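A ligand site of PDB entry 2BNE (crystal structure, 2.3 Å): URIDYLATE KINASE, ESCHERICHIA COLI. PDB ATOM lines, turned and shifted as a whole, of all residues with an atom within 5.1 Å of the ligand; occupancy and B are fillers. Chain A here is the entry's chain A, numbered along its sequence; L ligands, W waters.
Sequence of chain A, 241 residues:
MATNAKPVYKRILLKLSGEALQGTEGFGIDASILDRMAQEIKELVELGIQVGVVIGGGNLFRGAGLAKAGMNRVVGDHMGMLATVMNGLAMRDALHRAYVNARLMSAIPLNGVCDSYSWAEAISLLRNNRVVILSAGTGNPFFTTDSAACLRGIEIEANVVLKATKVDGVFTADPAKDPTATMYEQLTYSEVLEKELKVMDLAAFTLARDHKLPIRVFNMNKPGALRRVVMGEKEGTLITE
O7 of the ligand lies within salt-bridge range of NH1 of Arg 62 (3.2 Å). An oxygen (O6) of the ligand lies within hydrogen-bond range of the backbone NH of Gly 58 (3.2 Å). An oxygen (O2) of the ligand is in hydrogen-bond range of the backbone NH (N) of Thr 138, at 2.7 Å. A nitrogen (N2) of the ligand lies close to the backbone carbonyl oxygen (O) of Phe 143 (3.1 Å). N of Thr 145 sits at hydrogen-bond distance from O8 of the ligand, at 2.9 Å. The side-chain hydroxyl (OG1) of Thr 145 lies within hydrogen-bond range of an oxygen (O8) of the ligand (3.0 Å). O3 of the ligand lies within hydrogen-bond range of N of Gly 63, 2.7 Å away. OD1 of Asp 77 sits at hydrogen-bond distance from O3 of the ligand (2.7 Å). A nitrogen (N2) of the ligand is in hydrogen-bond range of the backbone carbonyl oxygen of Asn 140 (2.6 Å). O5 of the ligand sits at hydrogen-bond distance from N of Met 81. The side-chain hydroxyl of Thr 138 is in hydrogen-bond range of an oxygen (O2) of the ligand, at 2.6 Å. An oxygen (O9) of the ligand sits at hydrogen-bond distance from the backbone NH of Gly 57, at 2.8 Å.
The guanidinium group (NH2) of Arg 62 lies within hydrogen-bond range of the backbone carbonyl oxygen (O) of Gly 58 (3.3 Å). N of Asn 140 sits at hydrogen-bond distance from OG1 of Thr 138 (3.1 Å). NH2 of Arg 62 is in salt-bridge range of OE2 of Glu 19. The side-chain hydroxyl of Thr 144 lies close to the backbone NH of Asp 146. The backbone NH of Phe 142 is in hydrogen-bond range of the side-chain carboxylate of Asp 77 (2.7 Å). N of Asn 140 sits at hydrogen-bond distance from SD of Met 81 (3.7 Å). The backbone NH of Ala 136 lies within hydrogen-bond range of the side-chain hydroxyl of Thr 84 (2.5 Å). The backbone carbonyl oxygen (O) of Met 81 is in hydrogen-bond range of the side-chain hydroxyl (OG1) of Thr 84 (2.5 Å).
O of Gly 80 sits close to O5 of the ligand (3.5 Å). Residues that only touch the ligand: Gly 56, Thr 144, Pro 141, Gly 137, Gly 139, Thr 84, Phe 142 and Phe 61. Hydrophobic or aromatic side chains that line the ligand: Met 81 and Phe 143. 19 residues have an atom within 4 Å of the ligand: Gly 56, Gly 57, Gly 58, Phe 61, Arg 62, Gly 63, Asp 77, Gly 80, Met 81, Thr 84, Gly 137, Thr 138, Gly 139, Asn 140, Pro 141, Phe 142, Phe 143, Thr 144 and Thr 145. The nearest printed residue that does not touch the ligand is Ala 136 (4.2 Å).
Water W1 lies within hydrogen-bond range of O9 of the ligand (2.5 Å), NZ of Lys 15 (2.7 Å) and OG1 of Thr 145 (3.1 Å). Water W2 lies within hydrogen-bond range of the backbone NH (N) of Ala 64 (2.7 Å), an oxygen (O4) of the ligand (2.9 Å) and the backbone NH (N) of Gly 63 (2.9 Å). Water W3 lies within hydrogen-bond range of OG1 of Thr 145 (3.0 Å), N of Asp 146 (3.1 Å), NZ of Lys 15 (3.1 Å) and O8 of the ligand (3.4 Å).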
ATOM      1  N   LYS A  15      19.831  10.687 -19.650  1.00  0.00           N
ATOM      2  CA  LYS A  15      20.196  11.973 -20.238  1.00  0.00           C
ATOM      3  C   LYS A  15      21.623  12.313 -19.841  1.00  0.00           C
ATOM      4  O   LYS A  15      21.915  12.584 -18.679  1.00  0.00           O
ATOM      5  CB  LYS A  15      19.261  13.078 -19.776  1.00  0.00           C
ATOM      6  CG  LYS A  15      19.288  14.304 -20.661  1.00  0.00           C
ATOM      7  CD  LYS A  15      20.432  15.243 -20.345  1.00  0.00           C
ATOM      8  CE  LYS A  15      20.448  16.399 -21.337  1.00  0.00           C
ATOM      9  NZ  LYS A  15      21.157  17.584 -20.816  1.00  0.00           N
ATOM     10  N   GLY A  18      26.340  17.105 -22.322  1.00  0.00           N
ATOM     11  CA  GLY A  18      27.541  17.104 -23.136  1.00  0.00           C
ATOM     12  C   GLY A  18      28.836  17.338 -22.386  1.00  0.00           C
ATOM     13  O   GLY A  18      29.870  16.790 -22.752  1.00  0.00           O
ATOM     14  N   GLU A  19      28.795  18.129 -21.318  1.00  0.00           N
ATOM     15  CA  GLU A  19      30.014  18.414 -20.573  1.00  0.00           C
ATOM     16  C   GLU A  19      30.564  17.169 -19.878  1.00  0.00           C
ATOM     17  O   GLU A  19      31.752  17.117 -19.539  1.00  0.00           O
ATOM     18  CB  GLU A  19      29.750  19.513 -19.537  1.00  0.00           C
ATOM     19  CG  GLU A  19      29.171  20.803 -20.128  1.00  0.00           C
ATOM     20  CD  GLU A  19      27.742  20.627 -20.600  1.00  0.00           C
ATOM     21  OE1 GLU A  19      26.864  20.311 -19.755  1.00  0.00           O
ATOM     22  OE2 GLU A  19      27.479  20.808 -21.813  1.00  0.00           O
ATOM     23  N   GLY A  56      23.697  15.311 -24.842  1.00  0.00           N
ATOM     24  CA  GLY A  56      23.849  16.734 -25.024  1.00  0.00           C
ATOM     25  C   GLY A  56      24.889  17.084 -26.063  1.00  0.00           C
ATOM     26  O   GLY A  56      25.429  16.199 -26.726  1.00  0.00           O
ATOM     27  N   GLY A  57      25.167  18.368 -26.212  1.00  0.00           N
ATOM     28  CA  GLY A  57      26.161  18.802 -27.180  1.00  0.00           C
ATOM     29  C   GLY A  57      26.949  20.010 -26.706  1.00  0.00           C
ATOM     30  O   GLY A  57      27.899  20.447 -27.354  1.00  0.00           O
ATOM     31  N   GLY A  58      26.559  20.543 -25.550  1.00  0.00           N
ATOM     32  CA  GLY A  58      27.235  21.708 -25.002  1.00  0.00           C
ATOM     33  C   GLY A  58      28.734  21.613 -24.799  1.00  0.00           C
ATOM     34  O   GLY A  58      29.372  22.599 -24.473  1.00  0.00           O
ATOM     35  N   PHE A  61      29.152  22.796 -28.900  1.00  0.00           N
ATOM     36  CA  PHE A  61      28.495  24.046 -29.270  1.00  0.00           C
ATOM     37  C   PHE A  61      27.152  24.282 -28.581  1.00  0.00           C
ATOM     38  O   PHE A  61      26.384  23.359 -28.370  1.00  0.00           O
ATOM     39  CB  PHE A  61      28.256  24.117 -30.789  1.00  0.00           C
ATOM     40  CG  PHE A  61      29.512  24.207 -31.607  1.00  0.00           C
ATOM     41  CD1 PHE A  61      29.980  23.097 -32.303  1.00  0.00           C
ATOM     42  CD2 PHE A  61      30.203  25.414 -31.713  1.00  0.00           C
ATOM     43  CE1 PHE A  61      31.125  23.186 -33.096  1.00  0.00           C
ATOM     44  CE2 PHE A  61      31.343  25.507 -32.499  1.00  0.00           C
ATOM     45  CZ  PHE A  61      31.803  24.393 -33.199  1.00  0.00           C
ATOM     46  N   ARG A  62      26.897  25.537 -28.235  1.00  0.00           N
ATOM     47  CA  ARG A  62      25.643  25.935 -27.631  1.00  0.00           C
ATOM     48  C   ARG A  62      25.126  27.054 -28.536  1.00  0.00           C
ATOM     49  O   ARG A  62      25.803  28.065 -28.727  1.00  0.00           O
ATOM     50  CB  ARG A  62      25.835  26.471 -26.209  1.00  0.00           C
ATOM     51  CG  ARG A  62      26.345  25.442 -25.221  1.00  0.00           C
ATOM     52  CD  ARG A  62      26.501  26.063 -23.829  1.00  0.00           C
ATOM     53  NE  ARG A  62      27.345  25.260 -22.949  1.00  0.00           N
ATOM     54  CZ  ARG A  62      27.008  24.058 -22.479  1.00  0.00           C
ATOM     55  NH1 ARG A  62      25.840  23.505 -22.799  1.00  0.00           N
ATOM     56  NH2 ARG A  62      27.848  23.403 -21.681  1.00  0.00           N
ATOM     57  N   GLY A  63      23.950  26.851 -29.114  1.00  0.00           N
ATOM     58  CA  GLY A  63      23.375  27.838 -30.007  1.00  0.00           C
ATOM     59  C   GLY A  63      23.379  29.224 -29.395  1.00  0.00           C
ATOM     60  O   GLY A  63      23.883  30.174 -30.000  1.00  0.00           O
ATOM     61  N   ALA A  64      22.824  29.339 -28.201  1.00  0.00           N
ATOM     62  CA  ALA A  64      22.770  30.619 -27.509  1.00  0.00           C
ATOM     63  C   ALA A  64      24.146  31.261 -27.474  1.00  0.00           C
ATOM     64  O   ALA A  64      24.290  32.450 -27.771  1.00  0.00           O
ATOM     65  CB  ALA A  64      22.241  30.424 -26.091  1.00  0.00           C
ATOM     66  N   GLY A  76      22.829  28.612 -35.070  1.00  0.00           N
ATOM     67  CA  GLY A  76      23.604  28.250 -33.901  1.00  0.00           C
ATOM     68  C   GLY A  76      23.025  27.000 -33.278  1.00  0.00           C
ATOM     69  O   GLY A  76      23.770  26.111 -32.839  1.00  0.00           O
ATOM     70  N   ASP A  77      21.701  26.932 -33.207  1.00  0.00           N
ATOM     71  CA  ASP A  77      21.027  25.781 -32.626  1.00  0.00           C
ATOM     72  C   ASP A  77      21.184  24.550 -33.524  1.00  0.00           C
ATOM     73  O   ASP A  77      21.253  23.422 -33.027  1.00  0.00           O
ATOM     74  CB  ASP A  77      19.536  26.076 -32.383  1.00  0.00           C
ATOM     75  CG  ASP A  77      19.300  26.915 -31.134  1.00  0.00           C
ATOM     76  OD1 ASP A  77      20.195  26.977 -30.260  1.00  0.00           O
ATOM     77  OD2 ASP A  77      18.210  27.509 -31.012  1.00  0.00           O
ATOM     78  N   GLY A  80      24.409  23.235 -32.706  1.00  0.00           N
ATOM     79  CA  GLY A  80      24.324  22.589 -31.405  1.00  0.00           C
ATOM     80  C   GLY A  80      23.740  21.198 -31.559  1.00  0.00           C
ATOM     81  O   GLY A  80      24.243  20.234 -30.992  1.00  0.00           O
ATOM     82  N   MET A  81      22.660  21.091 -32.318  1.00  0.00           N
ATOM     83  CA  MET A  81      22.050  19.794 -32.526  1.00  0.00           C
ATOM     84  C   MET A  81      23.035  18.861 -33.219  1.00  0.00           C
ATOM     85  O   MET A  81      23.163  17.700 -32.824  1.00  0.00           O
ATOM     86  CB  MET A  81      20.755  19.929 -33.332  1.00  0.00           C
ATOM     87  CG  MET A  81      19.628  20.523 -32.502  1.00  0.00           C
ATOM     88  SD  MET A  81      18.037  20.518 -33.339  1.00  0.00           S
ATOM     89  CE  MET A  81      18.112  22.115 -34.177  1.00  0.00           C
ATOM     90  N   THR A  84      25.326  17.251 -30.913  1.00  0.00           N
ATOM     91  CA  THR A  84      24.805  16.115 -30.168  1.00  0.00           C
ATOM     92  C   THR A  84      24.919  14.845 -31.010  1.00  0.00           C
ATOM     93  O   THR A  84      25.076  13.751 -30.477  1.00  0.00           O
ATOM     94  CB  THR A  84      23.320  16.294 -29.762  1.00  0.00           C
ATOM     95  OG1 THR A  84      22.492  16.170 -30.921  1.00  0.00           O
ATOM     96  CG2 THR A  84      23.112  17.638 -29.113  1.00  0.00           C
ATOM     97  N   ALA A 136      20.337  15.068 -31.667  1.00  0.00           N
ATOM     98  CA  ALA A 136      19.733  16.255 -32.278  1.00  0.00           C
ATOM     99  C   ALA A 136      18.519  16.660 -31.455  1.00  0.00           C
ATOM    100  O   ALA A 136      17.622  17.345 -31.946  1.00  0.00           O
ATOM    101  CB  ALA A 136      19.327  15.978 -33.715  1.00  0.00           C
ATOM    102  N   GLY A 137      18.504  16.206 -30.203  1.00  0.00           N
ATOM    103  CA  GLY A 137      17.423  16.545 -29.299  1.00  0.00           C
ATOM    104  C   GLY A 137      16.026  16.493 -29.880  1.00  0.00           C
ATOM    105  O   GLY A 137      15.591  15.462 -30.382  1.00  0.00           O
ATOM    106  N   THR A 138      15.308  17.603 -29.814  1.00  0.00           N
ATOM    107  CA  THR A 138      13.941  17.676 -30.314  1.00  0.00           C
ATOM    108  C   THR A 138      13.920  17.992 -31.795  1.00  0.00           C
ATOM    109  O   THR A 138      12.862  17.948 -32.420  1.00  0.00           O
ATOM    110  CB  THR A 138      13.165  18.783 -29.607  1.00  0.00           C
ATOM    111  OG1 THR A 138      13.628  20.053 -30.085  1.00  0.00           O
ATOM    112  CG2 THR A 138      13.368  18.720 -28.093  1.00  0.00           C
ATOM    113  N   GLY A 139      15.068  18.336 -32.352  1.00  0.00           N
ATOM    114  CA  GLY A 139      15.103  18.665 -33.769  1.00  0.00           C
ATOM    115  C   GLY A 139      14.768  20.122 -34.029  1.00  0.00           C
ATOM    116  O   GLY A 139      14.910  20.609 -35.145  1.00  0.00           O
ATOM    117  N   ASN A 140      14.334  20.840 -32.990  1.00  0.00           N
ATOM    118  CA  ASN A 140      13.998  22.246 -33.155  1.00  0.00           C
ATOM    119  C   ASN A 140      14.881  23.201 -32.380  1.00  0.00           C
ATOM    120  O   ASN A 140      15.324  22.886 -31.272  1.00  0.00           O
ATOM    121  CB  ASN A 140      12.545  22.506 -32.728  1.00  0.00           C
ATOM    122  CG  ASN A 140      11.552  21.842 -33.633  1.00  0.00           C
ATOM    123  OD1 ASN A 140      11.663  21.921 -34.846  1.00  0.00           O
ATOM    124  ND2 ASN A 140      10.560  21.176 -33.047  1.00  0.00           N
ATOM    125  N   PRO A 141      15.148  24.381 -32.946  1.00  0.00           N
ATOM    126  CA  PRO A 141      15.982  25.378 -32.257  1.00  0.00           C
ATOM    127  C   PRO A 141      15.148  25.933 -31.099  1.00  0.00           C
ATOM    128  O   PRO A 141      13.939  25.725 -31.058  1.00  0.00           O
ATOM    129  CB  PRO A 141      16.229  26.427 -33.331  1.00  0.00           C
ATOM    130  CG  PRO A 141      14.958  26.383 -34.133  1.00  0.00           C
ATOM    131  CD  PRO A 141      14.763  24.879 -34.283  1.00  0.00           C
ATOM    132  N   PHE A 142      15.807  26.637 -30.185  1.00  0.00           N
ATOM    133  CA  PHE A 142      15.147  27.235 -29.039  1.00  0.00           C
ATOM    134  C   PHE A 142      14.785  26.239 -27.945  1.00  0.00           C
ATOM    135  O   PHE A 142      13.988  26.538 -27.048  1.00  0.00           O
ATOM    136  CB  PHE A 142      13.906  28.020 -29.477  1.00  0.00           C
ATOM    137  CG  PHE A 142      14.195  29.066 -30.517  1.00  0.00           C
ATOM    138  CD1 PHE A 142      15.117  30.071 -30.255  1.00  0.00           C
ATOM    139  CD2 PHE A 142      13.574  29.022 -31.748  1.00  0.00           C
ATOM    140  CE1 PHE A 142      15.412  31.028 -31.230  1.00  0.00           C
ATOM    141  CE2 PHE A 142      13.860  29.976 -32.728  1.00  0.00           C
ATOM    142  CZ  PHE A 142      14.783  30.980 -32.467  1.00  0.00           C
ATOM    143  N   PHE A 143      15.358  25.039 -28.021  1.00  0.00           N
ATOM    144  CA  PHE A 143      15.128  23.996 -27.020  1.00  0.00           C
ATOM    145  C   PHE A 143      16.474  23.422 -26.599  1.00  0.00           C
ATOM    146  O   PHE A 143      17.491  23.677 -27.250  1.00  0.00           O
ATOM    147  CB  PHE A 143      14.251  22.874 -27.580  1.00  0.00           C
ATOM    148  CG  PHE A 143      12.822  23.255 -27.744  1.00  0.00           C
ATOM    149  CD1 PHE A 143      12.428  24.119 -28.748  1.00  0.00           C
ATOM    150  CD2 PHE A 143      11.858  22.759 -26.871  1.00  0.00           C
ATOM    151  CE1 PHE A 143      11.091  24.506 -28.886  1.00  0.00           C
ATOM    152  CE2 PHE A 143      10.523  23.135 -26.987  1.00  0.00           C
ATOM    153  CZ  PHE A 143      10.134  24.013 -28.008  1.00  0.00           C
ATOM    154  N   THR A 144      16.470  22.644 -25.523  1.00  0.00           N
ATOM    155  CA  THR A 144      17.679  22.027 -25.007  1.00  0.00           C
ATOM    156  C   THR A 144      17.509  20.514 -25.051  1.00  0.00           C
ATOM    157  O   THR A 144      16.398  20.016 -25.274  1.00  0.00           O
ATOM    158  CB  THR A 144      17.911  22.433 -23.554  1.00  0.00           C
ATOM    159  OG1 THR A 144      16.861  21.901 -22.741  1.00  0.00           O
ATOM    160  CG2 THR A 144      17.939  23.957 -23.419  1.00  0.00           C
ATOM    161  N   THR A 145      18.596  19.767 -24.848  1.00  0.00           N
ATOM    162  CA  THR A 145      18.466  18.321 -24.856  1.00  0.00           C
ATOM    163  C   THR A 145      17.659  17.879 -23.644  1.00  0.00           C
ATOM    164  O   THR A 145      17.098  16.798 -23.629  1.00  0.00           O
ATOM    165  CB  THR A 145      19.844  17.614 -24.846  1.00  0.00           C
ATOM    166  OG1 THR A 145      20.635  18.099 -23.756  1.00  0.00           O
ATOM    167  CG2 THR A 145      20.581  17.856 -26.170  1.00  0.00           C
ATOM    168  N   ASP A 146      17.600  18.717 -22.614  1.00  0.00           N
ATOM    169  CA  ASP A 146      16.791  18.362 -21.450  1.00  0.00           C
ATOM    170  C   ASP A 146      15.327  18.236 -21.892  1.00  0.00           C
ATOM    171  O   ASP A 146      14.595  17.383 -21.390  1.00  0.00           O
ATOM    172  CB  ASP A 146      16.912  19.393 -20.328  1.00  0.00           C
ATOM    173  CG  ASP A 146      18.121  19.154 -19.438  1.00  0.00           C
ATOM    174  OD1 ASP A 146      18.725  18.062 -19.506  1.00  0.00           O
ATOM    175  OD2 ASP A 146      18.469  20.064 -18.652  1.00  0.00           O
ATOM    176  N   ALA A 148      14.382  17.377 -24.899  1.00  0.00           N
ATOM    177  CA  ALA A 148      14.342  16.162 -25.697  1.00  0.00           C
ATOM    178  C   ALA A 148      14.279  14.943 -24.775  1.00  0.00           C
ATOM    179  O   ALA A 148      13.566  13.983 -25.049  1.00  0.00           O
ATOM    180  CB  ALA A 148      15.586  16.071 -26.593  1.00  0.00           C
HETATM  181  N1  LIG L   1      19.497  22.317 -29.147  1.00  0.00           N
HETATM  182  C1  LIG L   1      18.388  22.788 -29.892  1.00  0.00           C
HETATM  183  N2  LIG L   1      17.270  21.977 -29.832  1.00  0.00           N
HETATM  184  C2  LIG L   1      17.108  20.792 -29.113  1.00  0.00           C
HETATM  185  C3  LIG L   1      18.249  20.412 -28.310  1.00  0.00           C
HETATM  186  C4  LIG L   1      19.371  21.159 -28.361  1.00  0.00           C
HETATM  187  O1  LIG L   1      18.421  23.830 -30.553  1.00  0.00           O
HETATM  188  O2  LIG L   1      16.071  20.159 -29.235  1.00  0.00           O
HETATM  189  C5  LIG L   1      20.790  22.999 -29.388  1.00  0.00           C
HETATM  190  C6  LIG L   1      21.119  24.145 -28.442  1.00  0.00           C
HETATM  191  O3  LIG L   1      21.826  25.170 -29.108  1.00  0.00           O
HETATM  192  C7  LIG L   1      21.928  23.451 -27.360  1.00  0.00           C
HETATM  193  C8  LIG L   1      22.658  22.367 -28.126  1.00  0.00           C
HETATM  194  O4  LIG L   1      22.828  24.325 -26.691  1.00  0.00           O
HETATM  195  O5  LIG L   1      21.866  22.114 -29.312  1.00  0.00           O
HETATM  196  C9  LIG L   1      22.786  21.060 -27.395  1.00  0.00           C
HETATM  197  O6  LIG L   1      23.482  21.267 -26.204  1.00  0.00           O
HETATM  198  P1  LIG L   1      22.782  21.121 -24.792  1.00  0.00           P
HETATM  199  O7  LIG L   1      23.160  22.285 -23.941  1.00  0.00           O
HETATM  200  O8  LIG L   1      21.347  20.726 -24.935  1.00  0.00           O
HETATM  201  O9  LIG L   1      23.622  19.815 -24.348  1.00  0.00           O
HETATM  202  O   HOH W   1      23.076  19.047 -22.040  1.00  0.00           O
HETATM  203  O   HOH W   2      22.179  27.156 -26.781  1.00  0.00           O
HETATM  204  O   HOH W   3      20.110  20.286 -21.827  1.00  0.00           O
